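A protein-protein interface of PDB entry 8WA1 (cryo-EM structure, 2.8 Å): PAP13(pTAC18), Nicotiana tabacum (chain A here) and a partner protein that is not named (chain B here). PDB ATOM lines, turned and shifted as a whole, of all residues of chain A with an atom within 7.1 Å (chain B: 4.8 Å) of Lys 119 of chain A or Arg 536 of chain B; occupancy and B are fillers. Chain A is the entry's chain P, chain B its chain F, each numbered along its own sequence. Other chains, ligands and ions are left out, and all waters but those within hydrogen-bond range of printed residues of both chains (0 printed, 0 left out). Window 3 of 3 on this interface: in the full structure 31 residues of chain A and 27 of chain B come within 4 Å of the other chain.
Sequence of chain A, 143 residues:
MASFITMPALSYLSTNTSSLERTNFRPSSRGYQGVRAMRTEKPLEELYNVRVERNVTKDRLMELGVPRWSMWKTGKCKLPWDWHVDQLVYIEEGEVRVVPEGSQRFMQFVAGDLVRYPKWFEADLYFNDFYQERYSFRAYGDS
The backbone carbonyl oxygen of Trp 83 of chain A is in hydrogen-bond range of the backbone NH of Trp 120 of chain A, 2.7 Å away. The backbone carbonyl oxygen (O) of His 84 of chain A lies close to the side-chain amino group (NZ) of Lys 119 of chain A (3.2 Å). OD1 of Asp 86 of chain A is in hydrogen-bond range of N of Lys 119 of chain A (3.0 Å). The side-chain carboxylate of Asp 532 of chain B lies within salt-bridge range of the guanidinium group of Arg 536 of chain B, at 2.9 Å. The backbone carbonyl oxygen (O) of Arg 536 of chain B sits at hydrogen-bond distance from the backbone NH (N) of Leu 541 of chain B, at 2.8 Å. The backbone carbonyl oxygen (O) of Pro 542 of chain B sits at hydrogen-bond distance from the guanidinium group (NE) of Arg 536 of chain B (3.3 Å).
Of the 17 printed residues of chain A, 5 touch a printed residue of chain B. Printed residues of chain A that touch a printed residue of chain B: Val 85, Lys 119, Trp 120, Ala 139 and Tyr 140. Hydrophobic or aromatic side chains of chain A within 4 Å of the printed part of chain B: Val 85, Trp 120, Ala 139 and Tyr 140. Along chain A the printed residues that touch a printed residue of chain B span positions 85 to 140. Printed residues of chain B that touch a printed residue of chain A: Asp 532, Arg 536, Leu 539, Leu 541 and Leu 543. Among the printed residues, no Asp or Glu carboxylate lies within 4 Å of a Lys or Arg side-chain nitrogen of the other chain.
NZ of Lys 119 of chain A is in hydrogen-bond range of O of Leu 543 of chain B, 3.3 Å away. O of Leu 543 of chain B lies close to NE1 of Trp 120 of chain A (3.1 Å).
Trp 83 of chain A touches none of the printed residues of chain B. Of the printed residues of chain B, Tyr 140 of chain A touches Asp 532, Leu 539 and Leu 541. Gly 141 of chain A touches none of the printed residues of chain B. Of the printed residues of chain A, Leu 541 of chain B touches Tyr 140. The nearest printed residue of chain B that does not touch Lys 119 of chain A is Pro 542 of chain B (5.6 Å). The nearest residue of chain A that does not touch Arg 536 of chain B is Trp 120 of chain A (4.1 Å).
Among the printed residues, merely in contact across the chains: Val 85 of chain A with Asp 532 of chain B, Lys 119 of chain A with Asp 532 of chain B, Tyr 140 of chain A with Leu 541 of chain B, Tyr 140 of chain A with Asp 532 of chain B, Lys 119 of chain A with Arg 536 of chain B, Ala 139 of chain A with Asp 532 of chain B and Tyr 140 of chain A with Leu 539 of chain B.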
ATOM      1  N   TYR A  48      10.086  20.498  35.370  1.00  0.00           N
ATOM      2  CA  TYR A  48       9.842  19.076  35.180  1.00  0.00           C
ATOM      3  C   TYR A  48       9.704  18.696  33.713  1.00  0.00           C
ATOM      4  O   TYR A  48       9.277  17.577  33.412  1.00  0.00           O
ATOM      5  CB  TYR A  48       8.597  18.645  35.957  1.00  0.00           C
ATOM      6  CG  TYR A  48       8.810  18.563  37.453  1.00  0.00           C
ATOM      7  CD1 TYR A  48       8.710  19.693  38.252  1.00  0.00           C
ATOM      8  CD2 TYR A  48       9.116  17.353  38.063  1.00  0.00           C
ATOM      9  CE1 TYR A  48       8.906  19.621  39.617  1.00  0.00           C
ATOM     10  CE2 TYR A  48       9.313  17.272  39.429  1.00  0.00           C
ATOM     11  CZ  TYR A  48       9.209  18.409  40.199  1.00  0.00           C
ATOM     12  OH  TYR A  48       9.403  18.332  41.559  1.00  0.00           O
ATOM     13  N   ASP A  82       2.856   6.956  38.209  1.00  0.00           N
ATOM     14  CA  ASP A  82       4.242   7.061  37.780  1.00  0.00           C
ATOM     15  C   ASP A  82       4.311   6.724  36.299  1.00  0.00           C
ATOM     16  O   ASP A  82       3.908   5.631  35.888  1.00  0.00           O
ATOM     17  CB  ASP A  82       5.149   6.120  38.580  1.00  0.00           C
ATOM     18  CG  ASP A  82       6.624   6.356  38.310  1.00  0.00           C
ATOM     19  OD1 ASP A  82       6.958   7.327  37.600  1.00  0.00           O
ATOM     20  OD2 ASP A  82       7.453   5.568  38.814  1.00  0.00           O
ATOM     21  N   TRP A  83       4.823   7.657  35.505  1.00  0.00           N
ATOM     22  CA  TRP A  83       4.896   7.494  34.060  1.00  0.00           C
ATOM     23  C   TRP A  83       6.164   6.732  33.703  1.00  0.00           C
ATOM     24  O   TRP A  83       7.268   7.279  33.790  1.00  0.00           O
ATOM     25  CB  TRP A  83       4.876   8.848  33.356  1.00  0.00           C
ATOM     26  CG  TRP A  83       3.514   9.438  33.218  1.00  0.00           C
ATOM     27  CD1 TRP A  83       2.681   9.330  32.144  1.00  0.00           C
ATOM     28  CD2 TRP A  83       2.821  10.236  34.184  1.00  0.00           C
ATOM     29  NE1 TRP A  83       1.513  10.012  32.380  1.00  0.00           N
ATOM     30  CE2 TRP A  83       1.574  10.576  33.627  1.00  0.00           C
ATOM     31  CE3 TRP A  83       3.135  10.695  35.467  1.00  0.00           C
ATOM     32  CZ2 TRP A  83       0.641  11.354  34.306  1.00  0.00           C
ATOM     33  CZ3 TRP A  83       2.207  11.467  36.140  1.00  0.00           C
ATOM     34  CH2 TRP A  83       0.976  11.789  35.558  1.00  0.00           C
ATOM     35  N   HIS A  84       6.001   5.474  33.301  1.00  0.00           N
ATOM     36  CA  HIS A  84       7.111   4.692  32.781  1.00  0.00           C
ATOM     37  C   HIS A  84       7.396   4.995  31.317  1.00  0.00           C
ATOM     38  O   HIS A  84       8.430   4.562  30.801  1.00  0.00           O
ATOM     39  CB  HIS A  84       6.832   3.195  32.949  1.00  0.00           C
ATOM     40  CG  HIS A  84       6.679   2.762  34.373  1.00  0.00           C
ATOM     41  ND1 HIS A  84       6.973   3.587  35.439  1.00  0.00           N
ATOM     42  CD2 HIS A  84       6.262   1.591  34.909  1.00  0.00           C
ATOM     43  CE1 HIS A  84       6.744   2.941  36.569  1.00  0.00           C
ATOM     44  NE2 HIS A  84       6.311   1.728  36.276  1.00  0.00           N
ATOM     45  N   VAL A  85       6.505   5.731  30.649  1.00  0.00           N
ATOM     46  CA  VAL A  85       6.691   6.156  29.267  1.00  0.00           C
ATOM     47  C   VAL A  85       6.034   7.516  29.105  1.00  0.00           C
ATOM     48  O   VAL A  85       5.260   7.961  29.956  1.00  0.00           O
ATOM     49  CB  VAL A  85       6.096   5.160  28.241  1.00  0.00           C
ATOM     50  CG1 VAL A  85       7.014   3.972  28.050  1.00  0.00           C
ATOM     51  CG2 VAL A  85       4.710   4.707  28.681  1.00  0.00           C
ATOM     52  N   ASP A  86       6.349   8.184  28.000  1.00  0.00           N
ATOM     53  CA  ASP A  86       5.714   9.455  27.699  1.00  0.00           C
ATOM     54  C   ASP A  86       4.253   9.239  27.318  1.00  0.00           C
ATOM     55  O   ASP A  86       3.894   8.252  26.671  1.00  0.00           O
ATOM     56  CB  ASP A  86       6.455  10.167  26.568  1.00  0.00           C
ATOM     57  CG  ASP A  86       7.920  10.391  26.885  1.00  0.00           C
ATOM     58  OD1 ASP A  86       8.245  10.609  28.071  1.00  0.00           O
ATOM     59  OD2 ASP A  86       8.747  10.345  25.950  1.00  0.00           O
ATOM     60  N   GLN A  87       3.406  10.177  27.732  1.00  0.00           N
ATOM     61  CA  GLN A  87       1.969  10.085  27.516  1.00  0.00           C
ATOM     62  C   GLN A  87       1.448  11.426  27.027  1.00  0.00           C
ATOM     63  O   GLN A  87       1.657  12.452  27.682  1.00  0.00           O
ATOM     64  CB  GLN A  87       1.243   9.674  28.802  1.00  0.00           C
ATOM     65  CG  GLN A  87      -0.267   9.580  28.666  1.00  0.00           C
ATOM     66  CD  GLN A  87      -0.960   9.389  30.002  1.00  0.00           C
ATOM     67  OE1 GLN A  87      -0.335   9.494  31.057  1.00  0.00           O
ATOM     68  NE2 GLN A  87      -2.256   9.105  29.963  1.00  0.00           N
ATOM     69  N   TYR A 117       3.268  14.186  29.344  1.00  0.00           N
ATOM     70  CA  TYR A 117       3.941  13.911  30.608  1.00  0.00           C
ATOM     71  C   TYR A 117       5.269  13.219  30.356  1.00  0.00           C
ATOM     72  O   TYR A 117       5.321  12.250  29.584  1.00  0.00           O
ATOM     73  CB  TYR A 117       3.064  13.041  31.504  1.00  0.00           C
ATOM     74  CG  TYR A 117       1.838  13.754  32.028  1.00  0.00           C
ATOM     75  CD1 TYR A 117       0.647  13.747  31.313  1.00  0.00           C
ATOM     76  CD2 TYR A 117       1.874  14.440  33.235  1.00  0.00           C
ATOM     77  CE1 TYR A 117      -0.475  14.401  31.789  1.00  0.00           C
ATOM     78  CE2 TYR A 117       0.756  15.095  33.718  1.00  0.00           C
ATOM     79  CZ  TYR A 117      -0.415  15.073  32.991  1.00  0.00           C
ATOM     80  OH  TYR A 117      -1.528  15.724  33.469  1.00  0.00           O
ATOM     81  N   PRO A 118       6.353  13.680  30.975  1.00  0.00           N
ATOM     82  CA  PRO A 118       7.667  13.085  30.712  1.00  0.00           C
ATOM     83  C   PRO A 118       7.817  11.720  31.367  1.00  0.00           C
ATOM     84  O   PRO A 118       7.010  11.298  32.199  1.00  0.00           O
ATOM     85  CB  PRO A 118       8.648  14.097  31.319  1.00  0.00           C
ATOM     86  CG  PRO A 118       7.840  15.342  31.565  1.00  0.00           C
ATOM     87  CD  PRO A 118       6.452  14.869  31.835  1.00  0.00           C
ATOM     88  N   LYS A 119       8.881  11.030  30.968  1.00  0.00           N
ATOM     89  CA  LYS A 119       9.208   9.732  31.541  1.00  0.00           C
ATOM     90  C   LYS A 119       9.721   9.891  32.969  1.00  0.00           C
ATOM     91  O   LYS A 119      10.287  10.922  33.339  1.00  0.00           O
ATOM     92  CB  LYS A 119      10.257   9.026  30.681  1.00  0.00           C
ATOM     93  CG  LYS A 119      10.343   7.521  30.878  1.00  0.00           C
ATOM     94  CD  LYS A 119      11.378   6.921  29.940  1.00  0.00           C
ATOM     95  CE  LYS A 119      11.366   5.401  29.986  1.00  0.00           C
ATOM     96  NZ  LYS A 119      11.585   4.879  31.362  1.00  0.00           N
ATOM     97  N   TRP A 120       9.506   8.848  33.775  1.00  0.00           N
ATOM     98  CA  TRP A 120       9.917   8.820  35.181  1.00  0.00           C
ATOM     99  C   TRP A 120       9.284   9.956  35.980  1.00  0.00           C
ATOM    100  O   TRP A 120       9.891  10.481  36.918  1.00  0.00           O
ATOM    101  CB  TRP A 120      11.443   8.862  35.327  1.00  0.00           C
ATOM    102  CG  TRP A 120      12.164   7.782  34.583  1.00  0.00           C
ATOM    103  CD1 TRP A 120      12.087   6.439  34.808  1.00  0.00           C
ATOM    104  CD2 TRP A 120      13.092   7.956  33.506  1.00  0.00           C
ATOM    105  NE1 TRP A 120      12.901   5.765  33.930  1.00  0.00           N
ATOM    106  CE2 TRP A 120      13.530   6.674  33.120  1.00  0.00           C
ATOM    107  CE3 TRP A 120      13.590   9.072  32.827  1.00  0.00           C
ATOM    108  CZ2 TRP A 120      14.442   6.478  32.086  1.00  0.00           C
ATOM    109  CZ3 TRP A 120      14.496   8.874  31.801  1.00  0.00           C
ATOM    110  CH2 TRP A 120      14.913   7.586  31.440  1.00  0.00           C
ATOM    111  N   PHE A 121       8.063  10.340  35.625  1.00  0.00           N
ATOM    112  CA  PHE A 121       7.352  11.413  36.306  1.00  0.00           C
ATOM    113  C   PHE A 121       6.495  10.823  37.417  1.00  0.00           C
ATOM    114  O   PHE A 121       5.648   9.962  37.163  1.00  0.00           O
ATOM    115  CB  PHE A 121       6.480  12.197  35.323  1.00  0.00           C
ATOM    116  CG  PHE A 121       6.000  13.521  35.853  1.00  0.00           C
ATOM    117  CD1 PHE A 121       6.543  14.063  37.008  1.00  0.00           C
ATOM    118  CD2 PHE A 121       5.003  14.222  35.197  1.00  0.00           C
ATOM    119  CE1 PHE A 121       6.102  15.277  37.495  1.00  0.00           C
ATOM    120  CE2 PHE A 121       4.558  15.439  35.681  1.00  0.00           C
ATOM    121  CZ  PHE A 121       5.109  15.967  36.831  1.00  0.00           C
ATOM    122  N   GLU A 122       6.718  11.289  38.644  1.00  0.00           N
ATOM    123  CA  GLU A 122       5.918  10.894  39.797  1.00  0.00           C
ATOM    124  C   GLU A 122       5.160  12.113  40.295  1.00  0.00           C
ATOM    125  O   GLU A 122       5.771  13.072  40.779  1.00  0.00           O
ATOM    126  CB  GLU A 122       6.794  10.308  40.908  1.00  0.00           C
ATOM    127  CG  GLU A 122       7.486   9.008  40.536  1.00  0.00           C
ATOM    128  CD  GLU A 122       8.101   8.313  41.735  1.00  0.00           C
ATOM    129  OE1 GLU A 122       7.995   8.853  42.856  1.00  0.00           O
ATOM    130  OE2 GLU A 122       8.687   7.224  41.558  1.00  0.00           O
ATOM    131  N   ARG A 138       3.249   6.979  24.158  1.00  0.00           N
ATOM    132  CA  ARG A 138       4.199   6.887  23.058  1.00  0.00           C
ATOM    133  C   ARG A 138       5.567   6.462  23.573  1.00  0.00           C
ATOM    134  O   ARG A 138       5.964   6.818  24.687  1.00  0.00           O
ATOM    135  CB  ARG A 138       4.318   8.222  22.317  1.00  0.00           C
ATOM    136  CG  ARG A 138       3.036   8.685  21.640  1.00  0.00           C
ATOM    137  CD  ARG A 138       3.296   9.905  20.765  1.00  0.00           C
ATOM    138  NE  ARG A 138       2.090  10.362  20.081  1.00  0.00           N
ATOM    139  CZ  ARG A 138       1.646   9.858  18.935  1.00  0.00           C
ATOM    140  NH1 ARG A 138       2.308   8.875  18.341  1.00  0.00           N
ATOM    141  NH2 ARG A 138       0.538  10.334  18.383  1.00  0.00           N
ATOM    142  N   ALA A 139       6.281   5.693  22.757  1.00  0.00           N
ATOM    143  CA  ALA A 139       7.633   5.261  23.065  1.00  0.00           C
ATOM    144  C   ALA A 139       8.634   6.283  22.529  1.00  0.00           C
ATOM    145  O   ALA A 139       8.269   7.366  22.065  1.00  0.00           O
ATOM    146  CB  ALA A 139       7.897   3.869  22.485  1.00  0.00           C
ATOM    147  N   TYR A 140       9.916   5.921  22.577  1.00  0.00           N
ATOM    148  CA  TYR A 140      10.958   6.797  22.057  1.00  0.00           C
ATOM    149  C   TYR A 140      10.720   7.076  20.578  1.00  0.00           C
ATOM    150  O   TYR A 140      10.729   6.164  19.746  1.00  0.00           O
ATOM    151  CB  TYR A 140      12.335   6.167  22.268  1.00  0.00           C
ATOM    152  CG  TYR A 140      13.473   7.000  21.727  1.00  0.00           C
ATOM    153  CD1 TYR A 140      14.001   8.049  22.466  1.00  0.00           C
ATOM    154  CD2 TYR A 140      14.015   6.739  20.478  1.00  0.00           C
ATOM    155  CE1 TYR A 140      15.038   8.816  21.975  1.00  0.00           C
ATOM    156  CE2 TYR A 140      15.052   7.500  19.976  1.00  0.00           C
ATOM    157  CZ  TYR A 140      15.560   8.537  20.730  1.00  0.00           C
ATOM    158  OH  TYR A 140      16.593   9.299  20.238  1.00  0.00           O
ATOM    159  N   GLY A 141      10.520   8.346  20.255  1.00  0.00           N
ATOM    160  CA  GLY A 141      10.042   8.765  18.953  1.00  0.00           C
ATOM    161  C   GLY A 141       8.603   9.247  19.027  1.00  0.00           C
ATOM    162  O   GLY A 141       8.114   9.699  20.065  1.00  0.00           O
ATOM    163  N   ASP B 532       9.130   0.728  24.236  1.00  0.00           N
ATOM    164  CA  ASP B 532      10.101   1.730  24.659  1.00  0.00           C
ATOM    165  C   ASP B 532      11.360   1.077  25.214  1.00  0.00           C
ATOM    166  O   ASP B 532      12.477   1.518  24.920  1.00  0.00           O
ATOM    167  CB  ASP B 532       9.476   2.660  25.696  1.00  0.00           C
ATOM    168  CG  ASP B 532      10.357   3.853  26.016  1.00  0.00           C
ATOM    169  OD1 ASP B 532      11.373   4.054  25.317  1.00  0.00           O
ATOM    170  OD2 ASP B 532      10.034   4.592  26.968  1.00  0.00           O
ATOM    171  N   ILE B 533      11.162  -0.056  25.878  1.00  0.00           N
ATOM    172  CA  ILE B 533      12.289  -0.795  26.426  1.00  0.00           C
ATOM    173  C   ILE B 533      13.132  -1.213  25.261  1.00  0.00           C
ATOM    174  O   ILE B 533      14.332  -0.989  25.248  1.00  0.00           O
ATOM    175  CB  ILE B 533      11.830  -2.051  27.198  1.00  0.00           C
ATOM    176  CG1 ILE B 533      11.321  -1.692  28.595  1.00  0.00           C
ATOM    177  CG2 ILE B 533      12.949  -3.073  27.339  1.00  0.00           C
ATOM    178  CD1 ILE B 533      11.857  -0.394  29.157  1.00  0.00           C
ATOM    179  N   SER B 534      12.503  -1.772  24.245  1.00  0.00           N
ATOM    180  CA  SER B 534      13.284  -2.293  23.143  1.00  0.00           C
ATOM    181  C   SER B 534      14.017  -1.197  22.452  1.00  0.00           C
ATOM    182  O   SER B 534      15.207  -1.296  22.232  1.00  0.00           O
ATOM    183  CB  SER B 534      12.405  -2.998  22.139  1.00  0.00           C
ATOM    184  OG  SER B 534      13.103  -3.203  20.926  1.00  0.00           O
ATOM    185  N   CYS B 535      13.298  -0.151  22.097  1.00  0.00           N
ATOM    186  CA  CYS B 535      13.922   0.953  21.421  1.00  0.00           C
ATOM    187  C   CYS B 535      15.114   1.456  22.195  1.00  0.00           C
ATOM    188  O   CYS B 535      16.170   1.688  21.615  1.00  0.00           O
ATOM    189  CB  CYS B 535      12.933   2.098  21.266  1.00  0.00           C
ATOM    190  SG  CYS B 535      11.610   1.818  20.075  1.00  0.00           S
ATOM    191  N   ARG B 536      14.971   1.606  23.508  1.00  0.00           N
ATOM    192  CA  ARG B 536      16.037   2.204  24.256  1.00  0.00           C
ATOM    193  C   ARG B 536      17.174   1.231  24.264  1.00  0.00           C
ATOM    194  O   ARG B 536      18.303   1.607  24.006  1.00  0.00           O
ATOM    195  CB  ARG B 536      15.576   2.558  25.659  1.00  0.00           C
ATOM    196  CG  ARG B 536      14.876   3.901  25.726  1.00  0.00           C
ATOM    197  CD  ARG B 536      14.414   4.234  27.131  1.00  0.00           C
ATOM    198  NE  ARG B 536      14.657   5.636  27.450  1.00  0.00           N
ATOM    199  CZ  ARG B 536      13.840   6.632  27.127  1.00  0.00           C
ATOM    200  NH1 ARG B 536      12.715   6.389  26.470  1.00  0.00           N
ATOM    201  NH2 ARG B 536      14.147   7.877  27.460  1.00  0.00           N
ATOM    202  N   ARG B 537      16.887  -0.033  24.527  1.00  0.00           N
ATOM    203  CA  ARG B 537      17.972  -0.991  24.635  1.00  0.00           C
ATOM    204  C   ARG B 537      18.698  -1.118  23.330  1.00  0.00           C
ATOM    205  O   ARG B 537      19.917  -1.231  23.300  1.00  0.00           O
ATOM    206  CB  ARG B 537      17.490  -2.349  25.114  1.00  0.00           C
ATOM    207  CG  ARG B 537      17.089  -2.329  26.577  1.00  0.00           C
ATOM    208  CD  ARG B 537      17.070  -3.721  27.169  1.00  0.00           C
ATOM    209  NE  ARG B 537      18.404  -4.306  27.191  1.00  0.00           N
ATOM    210  CZ  ARG B 537      19.240  -4.218  28.220  1.00  0.00           C
ATOM    211  NH1 ARG B 537      18.878  -3.566  29.317  1.00  0.00           N
ATOM    212  NH2 ARG B 537      20.436  -4.785  28.153  1.00  0.00           N
ATOM    213  N   ALA B 538      17.949  -1.104  22.246  1.00  0.00           N
ATOM    214  CA  ALA B 538      18.562  -1.235  20.950  1.00  0.00           C
ATOM    215  C   ALA B 538      19.532  -0.107  20.756  1.00  0.00           C
ATOM    216  O   ALA B 538      20.663  -0.318  20.338  1.00  0.00           O
ATOM    217  CB  ALA B 538      17.503  -1.180  19.884  1.00  0.00           C
ATOM    218  N   LEU B 539      19.093   1.100  21.063  1.00  0.00           N
ATOM    219  CA  LEU B 539      19.929   2.276  20.861  1.00  0.00           C
ATOM    220  C   LEU B 539      20.830   2.579  22.051  1.00  0.00           C
ATOM    221  O   LEU B 539      21.503   3.614  22.051  1.00  0.00           O
ATOM    222  CB  LEU B 539      19.057   3.496  20.544  1.00  0.00           C
ATOM    223  CG  LEU B 539      18.246   3.406  19.248  1.00  0.00           C
ATOM    224  CD1 LEU B 539      17.459   4.684  19.008  1.00  0.00           C
ATOM    225  CD2 LEU B 539      19.157   3.106  18.068  1.00  0.00           C
ATOM    226  N   GLY B 540      20.845   1.722  23.071  1.00  0.00           N
ATOM    227  CA  GLY B 540      21.736   1.889  24.197  1.00  0.00           C
ATOM    228  C   GLY B 540      21.271   2.871  25.249  1.00  0.00           C
ATOM    229  O   GLY B 540      21.977   3.061  26.246  1.00  0.00           O
ATOM    230  N   LEU B 541      20.116   3.504  25.059  1.00  0.00           N
ATOM    231  CA  LEU B 541      19.624   4.470  26.022  1.00  0.00           C
ATOM    232  C   LEU B 541      19.254   3.778  27.332  1.00  0.00           C
ATOM    233  O   LEU B 541      18.801   2.631  27.336  1.00  0.00           O
ATOM    234  CB  LEU B 541      18.422   5.219  25.455  1.00  0.00           C
ATOM    235  CG  LEU B 541      18.692   6.034  24.188  1.00  0.00           C
ATOM    236  CD1 LEU B 541      17.419   6.706  23.699  1.00  0.00           C
ATOM    237  CD2 LEU B 541      19.788   7.063  24.435  1.00  0.00           C
ATOM    238  N   PRO B 542      19.451   4.456  28.463  1.00  0.00           N
ATOM    239  CA  PRO B 542      19.182   3.819  29.757  1.00  0.00           C
ATOM    240  C   PRO B 542      17.691   3.657  30.008  1.00  0.00           C
ATOM    241  O   PRO B 542      16.868   4.446  29.541  1.00  0.00           O
ATOM    242  CB  PRO B 542      19.817   4.786  30.763  1.00  0.00           C
ATOM    243  CG  PRO B 542      19.788   6.106  30.075  1.00  0.00           C
ATOM    244  CD  PRO B 542      20.000   5.814  28.615  1.00  0.00           C
ATOM    245  N   LEU B 543      17.352   2.619  30.771  1.00  0.00           N
ATOM    246  CA  LEU B 543      15.964   2.330  31.112  1.00  0.00           C
ATOM    247  C   LEU B 543      15.498   3.035  32.375  1.00  0.00           C
ATOM    248  O   LEU B 543      14.326   3.414  32.459  1.00  0.00           O
ATOM    249  CB  LEU B 543      15.760   0.824  31.282  1.00  0.00           C
ATOM    250  CG  LEU B 543      16.143  -0.048  30.088  1.00  0.00           C
ATOM    251  CD1 LEU B 543      15.569  -1.445  30.247  1.00  0.00           C
ATOM    252  CD2 LEU B 543      15.683   0.586  28.782  1.00  0.00           C
